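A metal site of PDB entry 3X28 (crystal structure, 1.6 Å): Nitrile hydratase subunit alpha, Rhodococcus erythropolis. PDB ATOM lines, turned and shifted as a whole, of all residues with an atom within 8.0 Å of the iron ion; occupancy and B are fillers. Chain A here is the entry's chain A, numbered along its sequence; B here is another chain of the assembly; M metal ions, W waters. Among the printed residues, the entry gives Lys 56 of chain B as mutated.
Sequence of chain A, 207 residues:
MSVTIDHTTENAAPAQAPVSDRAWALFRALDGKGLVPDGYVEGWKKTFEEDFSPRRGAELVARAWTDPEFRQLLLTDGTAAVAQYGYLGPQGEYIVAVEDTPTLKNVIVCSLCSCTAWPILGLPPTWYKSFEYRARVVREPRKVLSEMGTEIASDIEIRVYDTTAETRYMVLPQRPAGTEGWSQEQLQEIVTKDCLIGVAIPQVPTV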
ATOM      1  N   GLN A  91     -22.421  -7.142 -23.438  1.00  0.00           N
ATOM      2  CA  GLN A  91     -23.443  -6.840 -22.455  1.00  0.00           C
ATOM      3  C   GLN A  91     -24.780  -7.301 -22.956  1.00  0.00           C
ATOM      4  O   GLN A  91     -25.834  -6.773 -22.612  1.00  0.00           O
ATOM      5  CB  GLN A  91     -23.444  -5.336 -22.103  1.00  0.00           C
ATOM      6  CG  GLN A  91     -22.135  -4.865 -21.454  1.00  0.00           C
ATOM      7  CD  GLN A  91     -21.967  -5.562 -20.147  1.00  0.00           C
ATOM      8  OE1 GLN A  91     -22.891  -5.553 -19.339  1.00  0.00           O
ATOM      9  NE2 GLN A  91     -20.830  -6.216 -19.948  1.00  0.00           N
ATOM     10  N   VAL A 109     -33.692  -3.002 -13.548  1.00  0.00           N
ATOM     11  CA  VAL A 109     -32.702  -2.043 -13.104  1.00  0.00           C
ATOM     12  C   VAL A 109     -31.325  -2.716 -12.954  1.00  0.00           C
ATOM     13  O   VAL A 109     -31.251  -3.953 -12.876  1.00  0.00           O
ATOM     14  CB  VAL A 109     -33.193  -1.466 -11.709  1.00  0.00           C
ATOM     15  CG1 VAL A 109     -33.272  -2.568 -10.642  1.00  0.00           C
ATOM     16  CG2 VAL A 109     -32.301  -0.334 -11.221  1.00  0.00           C
ATOM     17  N   CYS A 110     -30.272  -1.893 -12.801  1.00  0.00           N
ATOM     18  CA  CYS A 110     -29.033  -2.314 -12.196  1.00  0.00           C
ATOM     19  C   CYS A 110     -28.770  -1.426 -10.936  1.00  0.00           C
ATOM     20  O   CYS A 110     -28.306  -0.282 -11.085  1.00  0.00           O
ATOM     21  CB  CYS A 110     -27.921  -2.148 -13.227  1.00  0.00           C
ATOM     22  SG  CYS A 110     -26.330  -2.656 -12.505  1.00  0.00           S
ATOM     23  N   SER A 111     -29.131  -1.867  -9.748  1.00  0.00           N
ATOM     24  CA  SER A 111     -29.024  -1.039  -8.564  1.00  0.00           C
ATOM     25  C   SER A 111     -27.548  -0.740  -8.275  1.00  0.00           C
ATOM     26  O   SER A 111     -27.287   0.348  -7.758  1.00  0.00           O
ATOM     27  CB  SER A 111     -29.688  -1.616  -7.361  1.00  0.00           C
ATOM     28  OG  SER A 111     -29.036  -2.746  -6.871  1.00  0.00           O
ATOM     29  N   LEU A 112     -26.635  -1.622  -8.668  1.00  0.00           N
ATOM     30  CA  LEU A 112     -25.215  -1.413  -8.340  1.00  0.00           C
ATOM     31  C   LEU A 112     -24.408  -0.578  -9.302  1.00  0.00           C
ATOM     32  O   LEU A 112     -23.306  -0.176  -8.940  1.00  0.00           O
ATOM     33  CB  LEU A 112     -24.586  -2.812  -8.195  1.00  0.00           C
ATOM     34  CG  LEU A 112     -25.126  -3.744  -7.055  1.00  0.00           C
ATOM     35  CD1 LEU A 112     -24.649  -5.178  -7.105  1.00  0.00           C
ATOM     36  CD2 LEU A 112     -24.738  -3.167  -5.714  1.00  0.00           C
ATOM     37  N   CSD A 113     -24.962  -0.281 -10.475  1.00  0.00           N
ATOM     38  CA  CSD A 113     -24.275   0.440 -11.577  1.00  0.00           C
ATOM     39  CB  CSD A 113     -23.016  -0.316 -11.973  1.00  0.00           C
ATOM     40  SG  CSD A 113     -23.209  -1.946 -12.499  1.00  0.00           S
ATOM     41  C   CSD A 113     -25.234   0.786 -12.718  1.00  0.00           C
ATOM     42  O   CSD A 113     -25.864   1.850 -12.685  1.00  0.00           O
ATOM     43  OD1 CSD A 113     -21.817  -2.296 -12.966  1.00  0.00           O
ATOM     44  OD2 CSD A 113     -23.471  -2.752 -11.194  1.00  0.00           O
ATOM     45  N   SER A 114     -25.306   0.012 -13.783  1.00  0.00           N
ATOM     46  CA  SER A 114     -26.066   0.485 -14.967  1.00  0.00           C
ATOM     47  C   SER A 114     -26.377  -0.658 -15.940  1.00  0.00           C
ATOM     48  O   SER A 114     -26.944  -0.462 -17.016  1.00  0.00           O
ATOM     49  CB  SER A 114     -25.244   1.500 -15.656  1.00  0.00           C
ATOM     50  OG  SER A 114     -24.073   0.771 -16.215  1.00  0.00           O
ATOM     51  N   CSO A 115     -26.053  -1.861 -15.517  1.00  0.00           N
ATOM     52  CA  CSO A 115     -26.133  -3.011 -16.347  1.00  0.00           C
ATOM     53  CB  CSO A 115     -25.910  -4.194 -15.486  1.00  0.00           C
ATOM     54  SG  CSO A 115     -24.416  -4.126 -14.507  1.00  0.00           S
ATOM     55  C   CSO A 115     -27.484  -3.075 -17.055  1.00  0.00           C
ATOM     56  O   CSO A 115     -28.594  -2.992 -16.463  1.00  0.00           O
ATOM     57  OD  CSO A 115     -23.254  -4.172 -15.604  1.00  0.00           O
ATOM     58  N   THR A 116     -27.349  -3.233 -18.381  1.00  0.00           N
ATOM     59  CA  THR A 116     -28.404  -3.206 -19.385  1.00  0.00           C
ATOM     60  C   THR A 116     -28.079  -4.117 -20.553  1.00  0.00           C
ATOM     61  O   THR A 116     -26.928  -4.218 -20.953  1.00  0.00           O
ATOM     62  CB  THR A 116     -28.392  -1.793 -19.912  1.00  0.00           C
ATOM     63  OG1 THR A 116     -28.859  -0.900 -18.871  1.00  0.00           O
ATOM     64  CG2 THR A 116     -29.221  -1.570 -21.139  1.00  0.00           C
ATOM     65  N   TRP A 118     -27.352  -4.021 -23.705  1.00  0.00           N
ATOM     66  CA  TRP A 118     -27.007  -3.003 -24.692  1.00  0.00           C
ATOM     67  C   TRP A 118     -27.476  -3.348 -26.125  1.00  0.00           C
ATOM     68  O   TRP A 118     -27.963  -2.437 -26.779  1.00  0.00           O
ATOM     69  CB  TRP A 118     -25.499  -2.735 -24.768  1.00  0.00           C
ATOM     70  CG  TRP A 118     -24.884  -2.124 -23.571  1.00  0.00           C
ATOM     71  CD1 TRP A 118     -25.520  -1.548 -22.495  1.00  0.00           C
ATOM     72  CD2 TRP A 118     -23.476  -1.995 -23.325  1.00  0.00           C
ATOM     73  NE1 TRP A 118     -24.563  -0.998 -21.605  1.00  0.00           N
ATOM     74  CE2 TRP A 118     -23.309  -1.227 -22.122  1.00  0.00           C
ATOM     75  CE3 TRP A 118     -22.354  -2.399 -24.049  1.00  0.00           C
ATOM     76  CZ2 TRP A 118     -22.038  -0.961 -21.570  1.00  0.00           C
ATOM     77  CZ3 TRP A 118     -21.077  -2.034 -23.552  1.00  0.00           C
ATOM     78  CH2 TRP A 118     -20.938  -1.301 -22.346  1.00  0.00           C
ATOM     79  N   PRO A 124     -27.887   2.346 -21.718  1.00  0.00           N
ATOM     80  CA  PRO A 124     -28.884   2.952 -20.813  1.00  0.00           C
ATOM     81  C   PRO A 124     -28.965   4.426 -20.912  1.00  0.00           C
ATOM     82  O   PRO A 124     -27.953   5.110 -21.113  1.00  0.00           O
ATOM     83  CB  PRO A 124     -28.359   2.553 -19.408  1.00  0.00           C
ATOM     84  CG  PRO A 124     -26.924   2.258 -19.573  1.00  0.00           C
ATOM     85  CD  PRO A 124     -26.758   1.686 -20.990  1.00  0.00           C
ATOM     86  N   TYR A 128     -31.868   6.026 -16.103  1.00  0.00           N
ATOM     87  CA  TYR A 128     -31.779   4.626 -15.640  1.00  0.00           C
ATOM     88  C   TYR A 128     -30.562   4.465 -14.747  1.00  0.00           C
ATOM     89  O   TYR A 128     -30.546   3.618 -13.830  1.00  0.00           O
ATOM     90  CB  TYR A 128     -31.724   3.690 -16.852  1.00  0.00           C
ATOM     91  CG  TYR A 128     -31.567   2.236 -16.575  1.00  0.00           C
ATOM     92  CD1 TYR A 128     -30.319   1.640 -16.437  1.00  0.00           C
ATOM     93  CD2 TYR A 128     -32.659   1.434 -16.466  1.00  0.00           C
ATOM     94  CE1 TYR A 128     -30.133   0.288 -16.244  1.00  0.00           C
ATOM     95  CE2 TYR A 128     -32.533   0.051 -16.311  1.00  0.00           C
ATOM     96  CZ  TYR A 128     -31.276  -0.534 -16.217  1.00  0.00           C
ATOM     97  OH  TYR A 128     -31.074  -1.859 -16.077  1.00  0.00           O
ATOM     98  N   LYS A 129     -29.531   5.212 -15.070  1.00  0.00           N
ATOM     99  CA  LYS A 129     -28.278   5.228 -14.269  1.00  0.00           C
ATOM    100  C   LYS A 129     -28.353   6.176 -13.097  1.00  0.00           C
ATOM    101  O   LYS A 129     -27.416   6.258 -12.281  1.00  0.00           O
ATOM    102  CB  LYS A 129     -27.145   5.711 -15.228  1.00  0.00           C
ATOM    103  CG  LYS A 129     -26.957   4.716 -16.336  1.00  0.00           C
ATOM    104  CD  LYS A 129     -25.880   5.075 -17.304  1.00  0.00           C
ATOM    105  CE  LYS A 129     -26.300   6.172 -18.254  1.00  0.00           C
ATOM    106  NZ  LYS A 129     -25.353   6.435 -19.382  1.00  0.00           N
ATOM    107  N   ARG A 134     -31.922   3.904  -9.229  1.00  0.00           N
ATOM    108  CA  ARG A 134     -31.172   2.797  -8.636  1.00  0.00           C
ATOM    109  C   ARG A 134     -31.570   2.558  -7.171  1.00  0.00           C
ATOM    110  O   ARG A 134     -31.620   1.466  -6.708  1.00  0.00           O
ATOM    111  CB  ARG A 134     -29.679   3.131  -8.758  1.00  0.00           C
ATOM    112  CG  ARG A 134     -29.133   2.966 -10.171  1.00  0.00           C
ATOM    113  CD  ARG A 134     -27.663   3.327 -10.376  1.00  0.00           C
ATOM    114  NE  ARG A 134     -26.836   2.662  -9.377  1.00  0.00           N
ATOM    115  CZ  ARG A 134     -25.671   3.075  -8.915  1.00  0.00           C
ATOM    116  NH1 ARG A 134     -25.023   4.131  -9.430  1.00  0.00           N
ATOM    117  NH2 ARG A 134     -25.115   2.322  -7.943  1.00  0.00           N
ATOM    118  N   ASP A 162     -33.169  -7.090 -10.670  1.00  0.00           N
ATOM    119  CA  ASP A 162     -31.947  -6.345 -10.475  1.00  0.00           C
ATOM    120  C   ASP A 162     -30.838  -7.091 -11.216  1.00  0.00           C
ATOM    121  O   ASP A 162     -30.552  -8.298 -10.907  1.00  0.00           O
ATOM    122  CB  ASP A 162     -31.694  -6.249  -8.948  1.00  0.00           C
ATOM    123  CG  ASP A 162     -30.674  -5.108  -8.589  1.00  0.00           C
ATOM    124  OD1 ASP A 162     -30.017  -4.582  -9.507  1.00  0.00           O
ATOM    125  OD2 ASP A 162     -30.512  -4.880  -7.350  1.00  0.00           O
ATOM    126  N   THR A 163     -30.174  -6.376 -12.125  1.00  0.00           N
ATOM    127  CA  THR A 163     -29.204  -6.951 -13.060  1.00  0.00           C
ATOM    128  C   THR A 163     -27.827  -7.026 -12.403  1.00  0.00           C
ATOM    129  O   THR A 163     -26.985  -6.185 -12.679  1.00  0.00           O
ATOM    130  CB  THR A 163     -29.195  -6.129 -14.382  1.00  0.00           C
ATOM    131  OG1 THR A 163     -30.550  -6.077 -14.872  1.00  0.00           O
ATOM    132  CG2 THR A 163     -28.315  -6.848 -15.397  1.00  0.00           C
ATOM    133  N   THR A 164     -27.643  -8.002 -11.508  1.00  0.00           N
ATOM    134  CA  THR A 164     -26.473  -8.109 -10.634  1.00  0.00           C
ATOM    135  C   THR A 164     -25.386  -9.080 -11.105  1.00  0.00           C
ATOM    136  O   THR A 164     -24.311  -9.083 -10.531  1.00  0.00           O
ATOM    137  CB  THR A 164     -26.927  -8.541  -9.229  1.00  0.00           C
ATOM    138  OG1 THR A 164     -27.770  -9.702  -9.392  1.00  0.00           O
ATOM    139  CG2 THR A 164     -27.728  -7.535  -8.459  1.00  0.00           C
ATOM    140  N   ALA A 165     -25.630  -9.864 -12.177  1.00  0.00           N
ATOM    141  CA  ALA A 165     -24.552 -10.757 -12.685  1.00  0.00           C
ATOM    142  C   ALA A 165     -24.501 -10.639 -14.210  1.00  0.00           C
ATOM    143  O   ALA A 165     -24.429  -9.501 -14.733  1.00  0.00           O
ATOM    144  CB  ALA A 165     -24.755 -12.150 -12.189  1.00  0.00           C
ATOM    145  N   ARG A 168     -28.872 -10.659 -18.912  1.00  0.00           N
ATOM    146  CA  ARG A 168     -29.247  -9.343 -19.431  1.00  0.00           C
ATOM    147  C   ARG A 168     -30.690  -9.518 -19.876  1.00  0.00           C
ATOM    148  O   ARG A 168     -30.998 -10.452 -20.576  1.00  0.00           O
ATOM    149  CB  ARG A 168     -28.378  -8.910 -20.557  1.00  0.00           C
ATOM    150  CG  ARG A 168     -26.967  -8.592 -20.053  1.00  0.00           C
ATOM    151  CD  ARG A 168     -26.856  -7.249 -19.359  1.00  0.00           C
ATOM    152  NE  ARG A 168     -25.542  -6.992 -18.766  1.00  0.00           N
ATOM    153  CZ  ARG A 168     -25.088  -7.545 -17.596  1.00  0.00           C
ATOM    154  NH1 ARG A 168     -25.802  -8.422 -16.899  1.00  0.00           N
ATOM    155  NH2 ARG A 168     -23.837  -7.310 -17.198  1.00  0.00           N
ATOM    156  N   TYR B  37     -16.063   3.717 -22.121  1.00  0.00           N
ATOM    157  CA  TYR B  37     -16.414   2.370 -22.541  1.00  0.00           C
ATOM    158  C   TYR B  37     -15.450   1.830 -23.582  1.00  0.00           C
ATOM    159  O   TYR B  37     -15.038   0.683 -23.515  1.00  0.00           O
ATOM    160  CB  TYR B  37     -17.842   2.323 -23.101  1.00  0.00           C
ATOM    161  CG  TYR B  37     -19.028   2.320 -22.104  1.00  0.00           C
ATOM    162  CD1 TYR B  37     -18.855   2.387 -20.751  1.00  0.00           C
ATOM    163  CD2 TYR B  37     -20.298   2.322 -22.608  1.00  0.00           C
ATOM    164  CE1 TYR B  37     -19.935   2.395 -19.872  1.00  0.00           C
ATOM    165  CE2 TYR B  37     -21.414   2.302 -21.765  1.00  0.00           C
ATOM    166  CZ  TYR B  37     -21.240   2.312 -20.412  1.00  0.00           C
ATOM    167  OH  TYR B  37     -22.413   2.313 -19.644  1.00  0.00           O
ATOM    168  N   LYS B  56     -15.823  -2.569 -12.564  1.00  0.00           N
ATOM    169  CA  LYS B  56     -16.897  -2.323 -11.595  1.00  0.00           C
ATOM    170  C   LYS B  56     -16.329  -2.005 -10.241  1.00  0.00           C
ATOM    171  O   LYS B  56     -16.797  -1.070  -9.557  1.00  0.00           O
ATOM    172  CB  LYS B  56     -17.869  -3.528 -11.529  1.00  0.00           C
ATOM    173  CG  LYS B  56     -18.672  -3.856 -12.792  1.00  0.00           C
ATOM    174  CD  LYS B  56     -19.678  -4.995 -12.714  1.00  0.00           C
ATOM    175  CE  LYS B  56     -20.468  -5.052 -14.009  1.00  0.00           C
ATOM    176  NZ  LYS B  56     -21.374  -6.185 -14.286  1.00  0.00           N
ATOM    177  N   TYR B  72     -22.098   9.725 -14.126  1.00  0.00           N
ATOM    178  CA  TYR B  72     -21.836   8.370 -14.550  1.00  0.00           C
ATOM    179  C   TYR B  72     -20.628   8.129 -15.479  1.00  0.00           C
ATOM    180  O   TYR B  72     -19.732   7.357 -15.201  1.00  0.00           O
ATOM    181  CB  TYR B  72     -23.124   7.781 -15.211  1.00  0.00           C
ATOM    182  CG  TYR B  72     -22.883   6.401 -15.707  1.00  0.00           C
ATOM    183  CD1 TYR B  72     -23.110   5.300 -14.904  1.00  0.00           C
ATOM    184  CD2 TYR B  72     -22.436   6.166 -17.026  1.00  0.00           C
ATOM    185  CE1 TYR B  72     -22.936   4.012 -15.329  1.00  0.00           C
ATOM    186  CE2 TYR B  72     -22.137   4.864 -17.432  1.00  0.00           C
ATOM    187  CZ  TYR B  72     -22.369   3.787 -16.607  1.00  0.00           C
ATOM    188  OH  TYR B  72     -22.179   2.483 -17.052  1.00  0.00           O
ATOM    189  N   TYR B  76     -16.375   6.271 -14.939  1.00  0.00           N
ATOM    190  CA  TYR B  76     -15.648   5.214 -15.728  1.00  0.00           C
ATOM    191  C   TYR B  76     -14.345   5.798 -16.336  1.00  0.00           C
ATOM    192  O   TYR B  76     -13.391   5.061 -16.408  1.00  0.00           O
ATOM    193  CB  TYR B  76     -16.605   4.630 -16.813  1.00  0.00           C
ATOM    194  CG  TYR B  76     -17.698   3.772 -16.102  1.00  0.00           C
ATOM    195  CD1 TYR B  76     -17.513   2.414 -15.698  1.00  0.00           C
ATOM    196  CD2 TYR B  76     -18.803   4.414 -15.529  1.00  0.00           C
ATOM    197  CE1 TYR B  76     -18.469   1.742 -14.902  1.00  0.00           C
ATOM    198  CE2 TYR B  76     -19.737   3.745 -14.762  1.00  0.00           C
ATOM    199  CZ  TYR B  76     -19.557   2.440 -14.447  1.00  0.00           C
ATOM    200  OH  TYR B  76     -20.517   1.913 -13.645  1.00  0.00           O
ATOM    201  N   ARG B 141     -21.023  -9.192  -5.970  1.00  0.00           N
ATOM    202  CA  ARG B 141     -22.217  -8.880  -6.796  1.00  0.00           C
ATOM    203  C   ARG B 141     -23.499  -9.252  -6.067  1.00  0.00           C
ATOM    204  O   ARG B 141     -24.406  -9.895  -6.568  1.00  0.00           O
ATOM    205  CB  ARG B 141     -22.069  -9.524  -8.157  1.00  0.00           C
ATOM    206  CG  ARG B 141     -21.017  -8.831  -9.028  1.00  0.00           C
ATOM    207  CD  ARG B 141     -21.166  -7.312  -9.185  1.00  0.00           C
ATOM    208  NE  ARG B 141     -22.365  -7.023  -9.939  1.00  0.00           N
ATOM    209  CZ  ARG B 141     -22.716  -5.783 -10.279  1.00  0.00           C
ATOM    210  NH1 ARG B 141     -22.047  -4.781  -9.748  1.00  0.00           N
ATOM    211  NH2 ARG B 141     -23.736  -5.572 -11.084  1.00  0.00           N
HETATM  212 FE    FE M   1     -24.686  -1.946 -14.019  1.00  0.00          FE
HETATM  213  O   HOH W   1     -23.281  -1.385 -15.341  1.00  0.00           O
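Water W1 lies within hydrogen-bond range of the side-chain hydroxyl of Ser 114 (2.5 Å), OD of CSO 115 (2.8 Å) and OD1 of CSD 113 (2.9 Å).
The iron ion is bound by water W1 (2.0 Å), N of CSO 115 (2.0 Å), N of Ser 114 (2.1 Å), SG of CSD 113 (2.1 Å), SG of CSO 115 (2.3 Å) and SG of Cys 110 (2.3 Å).
The guanidinium group (NH2) of Arg 141 of chain B lies close to SG of CSO 115 (3.8 Å).
The side-chain hydroxyl (OG) of Ser 114 lies within hydrogen-bond range of the side-chain hydroxyl (OH) of Tyr 72 of chain B (2.7 Å).
OD of CSO 115 lies within hydrogen-bond range of the side-chain amino group (NZ) of Lys 56 of chain B (3.1 Å).
OH of Tyr 128 lies within hydrogen-bond range of N of Cys 110 (3.4 Å).
OD2 of CSD 113 is in salt-bridge range of the guanidinium group of Arg 141 of chain B (2.8 Å).
SG of Cys 110 lies close to O of Thr 163 (3.6 Å).
O of Ser 114 lies within hydrogen-bond range of OG1 of Thr 116 (2.7 Å).
O of CSO 115 is in hydrogen-bond range of OH of Tyr 128, at 2.8 Å.
Within 4 Å of the iron ion: Cys 110, CSD 113, Ser 114 and CSO 115.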
